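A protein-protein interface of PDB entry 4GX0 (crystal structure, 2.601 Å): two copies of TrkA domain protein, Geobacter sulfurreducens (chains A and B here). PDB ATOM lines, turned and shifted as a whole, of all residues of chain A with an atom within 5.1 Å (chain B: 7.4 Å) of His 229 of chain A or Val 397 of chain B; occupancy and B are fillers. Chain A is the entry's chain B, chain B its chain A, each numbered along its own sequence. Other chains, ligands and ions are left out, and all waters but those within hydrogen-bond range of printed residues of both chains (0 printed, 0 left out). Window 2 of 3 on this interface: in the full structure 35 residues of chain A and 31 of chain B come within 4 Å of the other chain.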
ATOM      1  N   ASP A 202     -28.666  23.432  21.282  1.00  0.00           N
ATOM      2  CA  ASP A 202     -28.757  22.609  22.483  1.00  0.00           C
ATOM      3  C   ASP A 202     -30.050  22.850  23.271  1.00  0.00           C
ATOM      4  O   ASP A 202     -30.680  21.899  23.729  1.00  0.00           O
ATOM      5  CB  ASP A 202     -27.507  22.758  23.358  1.00  0.00           C
ATOM      6  CG  ASP A 202     -26.267  22.140  22.715  1.00  0.00           C
ATOM      7  OD1 ASP A 202     -25.139  22.497  23.116  1.00  0.00           O
ATOM      8  OD2 ASP A 202     -26.421  21.300  21.801  1.00  0.00           O
ATOM      9  N   VAL A 224     -24.770  17.466  20.060  1.00  0.00           N
ATOM     10  CA  VAL A 224     -24.533  18.580  20.977  1.00  0.00           C
ATOM     11  C   VAL A 224     -23.494  19.553  20.423  1.00  0.00           C
ATOM     12  O   VAL A 224     -22.492  19.140  19.840  1.00  0.00           O
ATOM     13  CB  VAL A 224     -24.102  18.094  22.376  1.00  0.00           C
ATOM     14  CG1 VAL A 224     -22.766  17.377  22.307  1.00  0.00           C
ATOM     15  CG2 VAL A 224     -24.024  19.265  23.337  1.00  0.00           C
ATOM     16  N   GLU A 226     -22.003  21.912  22.339  1.00  0.00           N
ATOM     17  CA  GLU A 226     -21.050  22.209  23.398  1.00  0.00           C
ATOM     18  C   GLU A 226     -20.969  21.028  24.359  1.00  0.00           C
ATOM     19  O   GLU A 226     -21.895  20.789  25.127  1.00  0.00           O
ATOM     20  CB  GLU A 226     -21.465  23.476  24.150  1.00  0.00           C
ATOM     21  CG  GLU A 226     -20.390  24.033  25.072  1.00  0.00           C
ATOM     22  CD  GLU A 226     -19.226  24.643  24.311  1.00  0.00           C
ATOM     23  OE1 GLU A 226     -19.413  25.037  23.139  1.00  0.00           O
ATOM     24  OE2 GLU A 226     -18.120  24.727  24.886  1.00  0.00           O
ATOM     25  N   PRO A 227     -19.852  20.287  24.315  1.00  0.00           N
ATOM     26  CA  PRO A 227     -19.620  19.048  25.066  1.00  0.00           C
ATOM     27  C   PRO A 227     -20.124  19.067  26.509  1.00  0.00           C
ATOM     28  O   PRO A 227     -20.469  18.014  27.042  1.00  0.00           O
ATOM     29  CB  PRO A 227     -18.099  18.918  25.039  1.00  0.00           C
ATOM     30  CG  PRO A 227     -17.723  19.500  23.723  1.00  0.00           C
ATOM     31  CD  PRO A 227     -18.688  20.640  23.480  1.00  0.00           C
ATOM     32  N   VAL A 228     -20.161  20.240  27.129  1.00  0.00           N
ATOM     33  CA  VAL A 228     -20.614  20.359  28.512  1.00  0.00           C
ATOM     34  C   VAL A 228     -22.119  20.110  28.644  1.00  0.00           C
ATOM     35  O   VAL A 228     -22.599  19.689  29.697  1.00  0.00           O
ATOM     36  CB  VAL A 228     -20.279  21.747  29.086  1.00  0.00           C
ATOM     37  CG1 VAL A 228     -20.415  21.741  30.602  1.00  0.00           C
ATOM     38  CG2 VAL A 228     -18.873  22.164  28.672  1.00  0.00           C
ATOM     39  N   HIS A 229     -22.855  20.372  27.568  1.00  0.00           N
ATOM     40  CA  HIS A 229     -24.305  20.201  27.545  1.00  0.00           C
ATOM     41  C   HIS A 229     -24.710  18.756  27.290  1.00  0.00           C
ATOM     42  O   HIS A 229     -25.896  18.426  27.308  1.00  0.00           O
ATOM     43  CB  HIS A 229     -24.925  21.087  26.464  1.00  0.00           C
ATOM     44  CG  HIS A 229     -24.680  22.548  26.663  1.00  0.00           C
ATOM     45  ND1 HIS A 229     -24.780  23.465  25.643  1.00  0.00           N
ATOM     46  CD2 HIS A 229     -24.343  23.251  27.771  1.00  0.00           C
ATOM     47  CE1 HIS A 229     -24.513  24.672  26.109  1.00  0.00           C
ATOM     48  NE2 HIS A 229     -24.246  24.569  27.397  1.00  0.00           N
ATOM     49  N   GLY A 230     -23.729  17.900  27.035  1.00  0.00           N
ATOM     50  CA  GLY A 230     -23.999  16.499  26.767  1.00  0.00           C
ATOM     51  C   GLY A 230     -24.824  15.846  27.859  1.00  0.00           C
ATOM     52  O   GLY A 230     -25.818  15.180  27.578  1.00  0.00           O
ATOM     53  N   GLU A 231     -24.408  16.037  29.107  1.00  0.00           N
ATOM     54  CA  GLU A 231     -25.109  15.463  30.250  1.00  0.00           C
ATOM     55  C   GLU A 231     -26.567  15.910  30.280  1.00  0.00           C
ATOM     56  O   GLU A 231     -27.471  15.097  30.463  1.00  0.00           O
ATOM     57  CB  GLU A 231     -24.420  15.867  31.555  1.00  0.00           C
ATOM     58  CG  GLU A 231     -22.929  15.570  31.594  1.00  0.00           C
ATOM     59  CD  GLU A 231     -22.257  16.113  32.844  1.00  0.00           C
ATOM     60  OE1 GLU A 231     -21.016  16.266  32.834  1.00  0.00           O
ATOM     61  OE2 GLU A 231     -22.969  16.388  33.835  1.00  0.00           O
ATOM     62  N   LEU A 232     -26.785  17.209  30.104  1.00  0.00           N
ATOM     63  CA  LEU A 232     -28.127  17.780  30.105  1.00  0.00           C
ATOM     64  C   LEU A 232     -29.058  17.133  29.074  1.00  0.00           C
ATOM     65  O   LEU A 232     -30.238  16.918  29.347  1.00  0.00           O
ATOM     66  CB  LEU A 232     -28.056  19.290  29.877  1.00  0.00           C
ATOM     67  CG  LEU A 232     -28.095  20.192  31.113  1.00  0.00           C
ATOM     68  CD1 LEU A 232     -27.570  19.474  32.342  1.00  0.00           C
ATOM     69  CD2 LEU A 232     -27.332  21.491  30.861  1.00  0.00           C
ATOM     70  N   LEU A 233     -28.529  16.821  27.894  1.00  0.00           N
ATOM     71  CA  LEU A 233     -29.336  16.207  26.840  1.00  0.00           C
ATOM     72  C   LEU A 233     -29.697  14.752  27.143  1.00  0.00           C
ATOM     73  O   LEU A 233     -30.783  14.292  26.793  1.00  0.00           O
ATOM     74  CB  LEU A 233     -28.636  16.315  25.483  1.00  0.00           C
ATOM     75  CG  LEU A 233     -29.034  17.501  24.600  1.00  0.00           C
ATOM     76  CD1 LEU A 233     -29.629  18.633  25.417  1.00  0.00           C
ATOM     77  CD2 LEU A 233     -27.843  17.988  23.792  1.00  0.00           C
ATOM     78  N   PRO A 383     -17.221  34.273  21.207  1.00  0.00           N
ATOM     79  CA  PRO A 383     -18.427  34.566  21.988  1.00  0.00           C
ATOM     80  C   PRO A 383     -18.757  33.452  22.975  1.00  0.00           C
ATOM     81  O   PRO A 383     -19.644  33.618  23.812  1.00  0.00           O
ATOM     82  CB  PRO A 383     -19.516  34.647  20.918  1.00  0.00           C
ATOM     83  CG  PRO A 383     -19.043  33.727  19.853  1.00  0.00           C
ATOM     84  CD  PRO A 383     -17.543  33.859  19.830  1.00  0.00           C
ATOM     85  N   VAL A 384     -18.047  32.332  22.882  1.00  0.00           N
ATOM     86  CA  VAL A 384     -18.358  31.173  23.710  1.00  0.00           C
ATOM     87  C   VAL A 384     -17.180  30.714  24.565  1.00  0.00           C
ATOM     88  O   VAL A 384     -17.369  30.113  25.622  1.00  0.00           O
ATOM     89  CB  VAL A 384     -18.870  29.996  22.854  1.00  0.00           C
ATOM     90  CG1 VAL A 384     -17.937  29.747  21.683  1.00  0.00           C
ATOM     91  CG2 VAL A 384     -19.021  28.744  23.704  1.00  0.00           C
ATOM     92  N   ARG B 379     -27.626  39.023  29.597  1.00  0.00           N
ATOM     93  CA  ARG B 379     -26.456  39.058  28.734  1.00  0.00           C
ATOM     94  C   ARG B 379     -26.307  40.430  28.091  1.00  0.00           C
ATOM     95  O   ARG B 379     -25.314  40.710  27.421  1.00  0.00           O
ATOM     96  CB  ARG B 379     -26.553  37.971  27.663  1.00  0.00           C
ATOM     97  CG  ARG B 379     -27.740  38.127  26.729  1.00  0.00           C
ATOM     98  CD  ARG B 379     -28.064  36.817  26.027  1.00  0.00           C
ATOM     99  NE  ARG B 379     -26.894  36.233  25.380  1.00  0.00           N
ATOM    100  CZ  ARG B 379     -26.907  35.082  24.715  1.00  0.00           C
ATOM    101  NH1 ARG B 379     -25.794  34.622  24.159  1.00  0.00           N
ATOM    102  NH2 ARG B 379     -28.033  34.389  24.609  1.00  0.00           N
ATOM    103  N   GLY B 393     -23.365  39.215  31.399  1.00  0.00           N
ATOM    104  CA  GLY B 393     -22.658  38.011  31.002  1.00  0.00           C
ATOM    105  C   GLY B 393     -23.619  36.858  30.793  1.00  0.00           C
ATOM    106  O   GLY B 393     -24.367  36.494  31.700  1.00  0.00           O
ATOM    107  N   ASP B 394     -23.598  36.285  29.592  1.00  0.00           N
ATOM    108  CA  ASP B 394     -24.503  35.194  29.236  1.00  0.00           C
ATOM    109  C   ASP B 394     -24.464  34.057  30.257  1.00  0.00           C
ATOM    110  O   ASP B 394     -23.416  33.770  30.834  1.00  0.00           O
ATOM    111  CB  ASP B 394     -24.172  34.661  27.840  1.00  0.00           C
ATOM    112  CG  ASP B 394     -25.011  33.457  27.463  1.00  0.00           C
ATOM    113  OD1 ASP B 394     -24.484  32.326  27.509  1.00  0.00           O
ATOM    114  OD2 ASP B 394     -26.199  33.641  27.125  1.00  0.00           O
ATOM    115  N   ALA B 395     -25.608  33.413  30.470  1.00  0.00           N
ATOM    116  CA  ALA B 395     -25.725  32.364  31.483  1.00  0.00           C
ATOM    117  C   ALA B 395     -25.732  30.954  30.893  1.00  0.00           C
ATOM    118  O   ALA B 395     -25.468  29.979  31.599  1.00  0.00           O
ATOM    119  CB  ALA B 395     -26.969  32.586  32.335  1.00  0.00           C
ATOM    120  N   THR B 396     -26.037  30.848  29.604  1.00  0.00           N
ATOM    121  CA  THR B 396     -26.131  29.547  28.945  1.00  0.00           C
ATOM    122  C   THR B 396     -24.761  28.873  28.808  1.00  0.00           C
ATOM    123  O   THR B 396     -24.671  27.650  28.694  1.00  0.00           O
ATOM    124  CB  THR B 396     -26.823  29.660  27.558  1.00  0.00           C
ATOM    125  OG1 THR B 396     -28.193  30.043  27.734  1.00  0.00           O
ATOM    126  CG2 THR B 396     -26.770  28.335  26.810  1.00  0.00           C
ATOM    127  N   VAL B 397     -23.699  29.673  28.842  1.00  0.00           N
ATOM    128  CA  VAL B 397     -22.338  29.165  28.665  1.00  0.00           C
ATOM    129  C   VAL B 397     -21.999  28.019  29.621  1.00  0.00           C
ATOM    130  O   VAL B 397     -21.587  26.943  29.187  1.00  0.00           O
ATOM    131  CB  VAL B 397     -21.288  30.298  28.794  1.00  0.00           C
ATOM    132  CG1 VAL B 397     -19.883  29.717  28.758  1.00  0.00           C
ATOM    133  CG2 VAL B 397     -21.482  31.321  27.683  1.00  0.00           C
ATOM    134  N   GLY B 398     -22.182  28.247  30.919  1.00  0.00           N
ATOM    135  CA  GLY B 398     -21.973  27.197  31.898  1.00  0.00           C
ATOM    136  C   GLY B 398     -21.825  27.663  33.335  1.00  0.00           C
ATOM    137  O   GLY B 398     -22.721  27.462  34.155  1.00  0.00           O
ATOM    138  N   GLN B 399     -20.691  28.288  33.635  1.00  0.00           N
ATOM    139  CA  GLN B 399     -20.327  28.603  35.013  1.00  0.00           C
ATOM    140  C   GLN B 399     -20.706  30.020  35.434  1.00  0.00           C
ATOM    141  O   GLN B 399     -20.339  30.470  36.518  1.00  0.00           O
ATOM    142  CB  GLN B 399     -18.828  28.384  35.225  1.00  0.00           C
ATOM    143  CG  GLN B 399     -17.942  29.326  34.424  1.00  0.00           C
ATOM    144  CD  GLN B 399     -16.474  29.112  34.718  1.00  0.00           C
ATOM    145  OE1 GLN B 399     -16.117  28.314  35.585  1.00  0.00           O
ATOM    146  NE2 GLN B 399     -15.612  29.821  33.999  1.00  0.00           N
ATOM    147  N   THR B 400     -21.442  30.719  34.576  1.00  0.00           N
ATOM    148  CA  THR B 400     -21.887  32.075  34.881  1.00  0.00           C
ATOM    149  C   THR B 400     -22.806  32.088  36.102  1.00  0.00           C
ATOM    150  O   THR B 400     -22.861  33.072  36.843  1.00  0.00           O
ATOM    151  CB  THR B 400     -22.610  32.705  33.678  1.00  0.00           C
ATOM    152  OG1 THR B 400     -21.771  32.618  32.520  1.00  0.00           O
ATOM    153  CG2 THR B 400     -22.939  34.166  33.951  1.00  0.00           C
ATOM    154  N   PHE B 424     -33.921  24.762  29.020  1.00  0.00           N
ATOM    155  CA  PHE B 424     -32.520  24.398  29.207  1.00  0.00           C
ATOM    156  C   PHE B 424     -31.996  24.876  30.562  1.00  0.00           C
ATOM    157  O   PHE B 424     -31.349  24.120  31.285  1.00  0.00           O
ATOM    158  CB  PHE B 424     -31.673  24.978  28.075  1.00  0.00           C
ATOM    159  CG  PHE B 424     -30.370  24.261  27.858  1.00  0.00           C
ATOM    160  CD1 PHE B 424     -30.351  22.965  27.368  1.00  0.00           C
ATOM    161  CD2 PHE B 424     -29.164  24.892  28.116  1.00  0.00           C
ATOM    162  CE1 PHE B 424     -29.153  22.306  27.155  1.00  0.00           C
ATOM    163  CE2 PHE B 424     -27.964  24.239  27.901  1.00  0.00           C
ATOM    164  CZ  PHE B 424     -27.959  22.944  27.420  1.00  0.00           C
ATOM    165  N   LEU B 425     -32.276  26.132  30.902  1.00  0.00           N
ATOM    166  CA  LEU B 425     -31.823  26.698  32.171  1.00  0.00           C
ATOM    167  C   LEU B 425     -32.426  25.945  33.354  1.00  0.00           C
ATOM    168  O   LEU B 425     -31.746  25.691  34.348  1.00  0.00           O
ATOM    169  CB  LEU B 425     -32.168  28.188  32.265  1.00  0.00           C
ATOM    170  CG  LEU B 425     -31.552  29.122  31.221  1.00  0.00           C
ATOM    171  CD1 LEU B 425     -32.020  30.544  31.461  1.00  0.00           C
ATOM    172  CD2 LEU B 425     -30.028  29.042  31.218  1.00  0.00           C
ATOM    173  N   ALA B 428     -30.518  22.647  33.680  1.00  0.00           N
ATOM    174  CA  ALA B 428     -29.198  22.892  34.249  1.00  0.00           C
ATOM    175  C   ALA B 428     -29.290  23.192  35.739  1.00  0.00           C
ATOM    176  O   ALA B 428     -28.512  22.670  36.532  1.00  0.00           O
ATOM    177  CB  ALA B 428     -28.505  24.032  33.515  1.00  0.00           C
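A ring nitrogen (NE2) of His 229 of chain A is in hydrogen-bond range of the backbone carbonyl oxygen of Thr 396 of chain B, at 3.4 Å.
The backbone NH (N) of Thr 396 of chain B lies within hydrogen-bond range of the side-chain carboxylate (OD1) of Asp 394 of chain B. OD1 of Asp 394 of chain B is in hydrogen-bond range of N of Val 397 of chain B (3.1 Å). The side-chain carboxylate (OD1) of Asp 202 of chain A sits at hydrogen-bond distance from the backbone NH (N) of Glu 226 of chain A. ND1 of His 229 of chain A lies within hydrogen-bond range of OD1 of Asp 202 of chain A (2.7 Å).
Among the printed residues, merely in contact across the chains: Asp 202 of chain A with Phe 424 of chain B (3.8 Å), His 229 of chain A with Val 397 of chain B (3.99 Å), His 229 of chain A with Phe 424 of chain B (3.4 Å), Leu 232 of chain A with Phe 424 of chain B (3.8 Å) and Leu 232 of chain A with Ala 428 of chain B (3.9 Å).
Printed residues of chain B within 4 Å of His 229 of chain A: Thr 396, Val 397 and Phe 424. Printed residues of chain A within 4 Å of Val 397 of chain B: His 229 (3.99 Å). No residue of chain B comes within 4 Å of Gly 230 of chain A. Of the printed residues of chain A, Phe 424 of chain B touches Asp 202, His 229 and Leu 232. Printed residues of chain A within 4 Å of Ala 428 of chain B: Leu 232. Printed residues of chain B within 4 Å of Leu 232 of chain A: Phe 424 and Ala 428. Asp 394 of chain B touches none of the printed residues of chain A. The nearest printed residue of chain B that does not touch His 229 of chain A is Gly 398 of chain B (5.5 Å). The nearest printed residue of chain B that does not touch Asp 202 of chain A is Thr 396 of chain B (6.6 Å).
Of the 12 printed residues of chain A, 3 touch a printed residue of chain B. Printed residues of chain A that touch a printed residue of chain B: Asp 202, His 229 and Leu 232. Of the 12 printed residues of chain B, 4 touch a printed residue of chain A. Hydrophobic or aromatic side chains of chain B within 4 Å of the printed part of chain A: Phe 424 and Ala 428. Among the printed residues, no Asp or Glu carboxylate lies within 4 Å of a Lys or Arg side-chain nitrogen of the other chain.
No position is printed for both chains.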
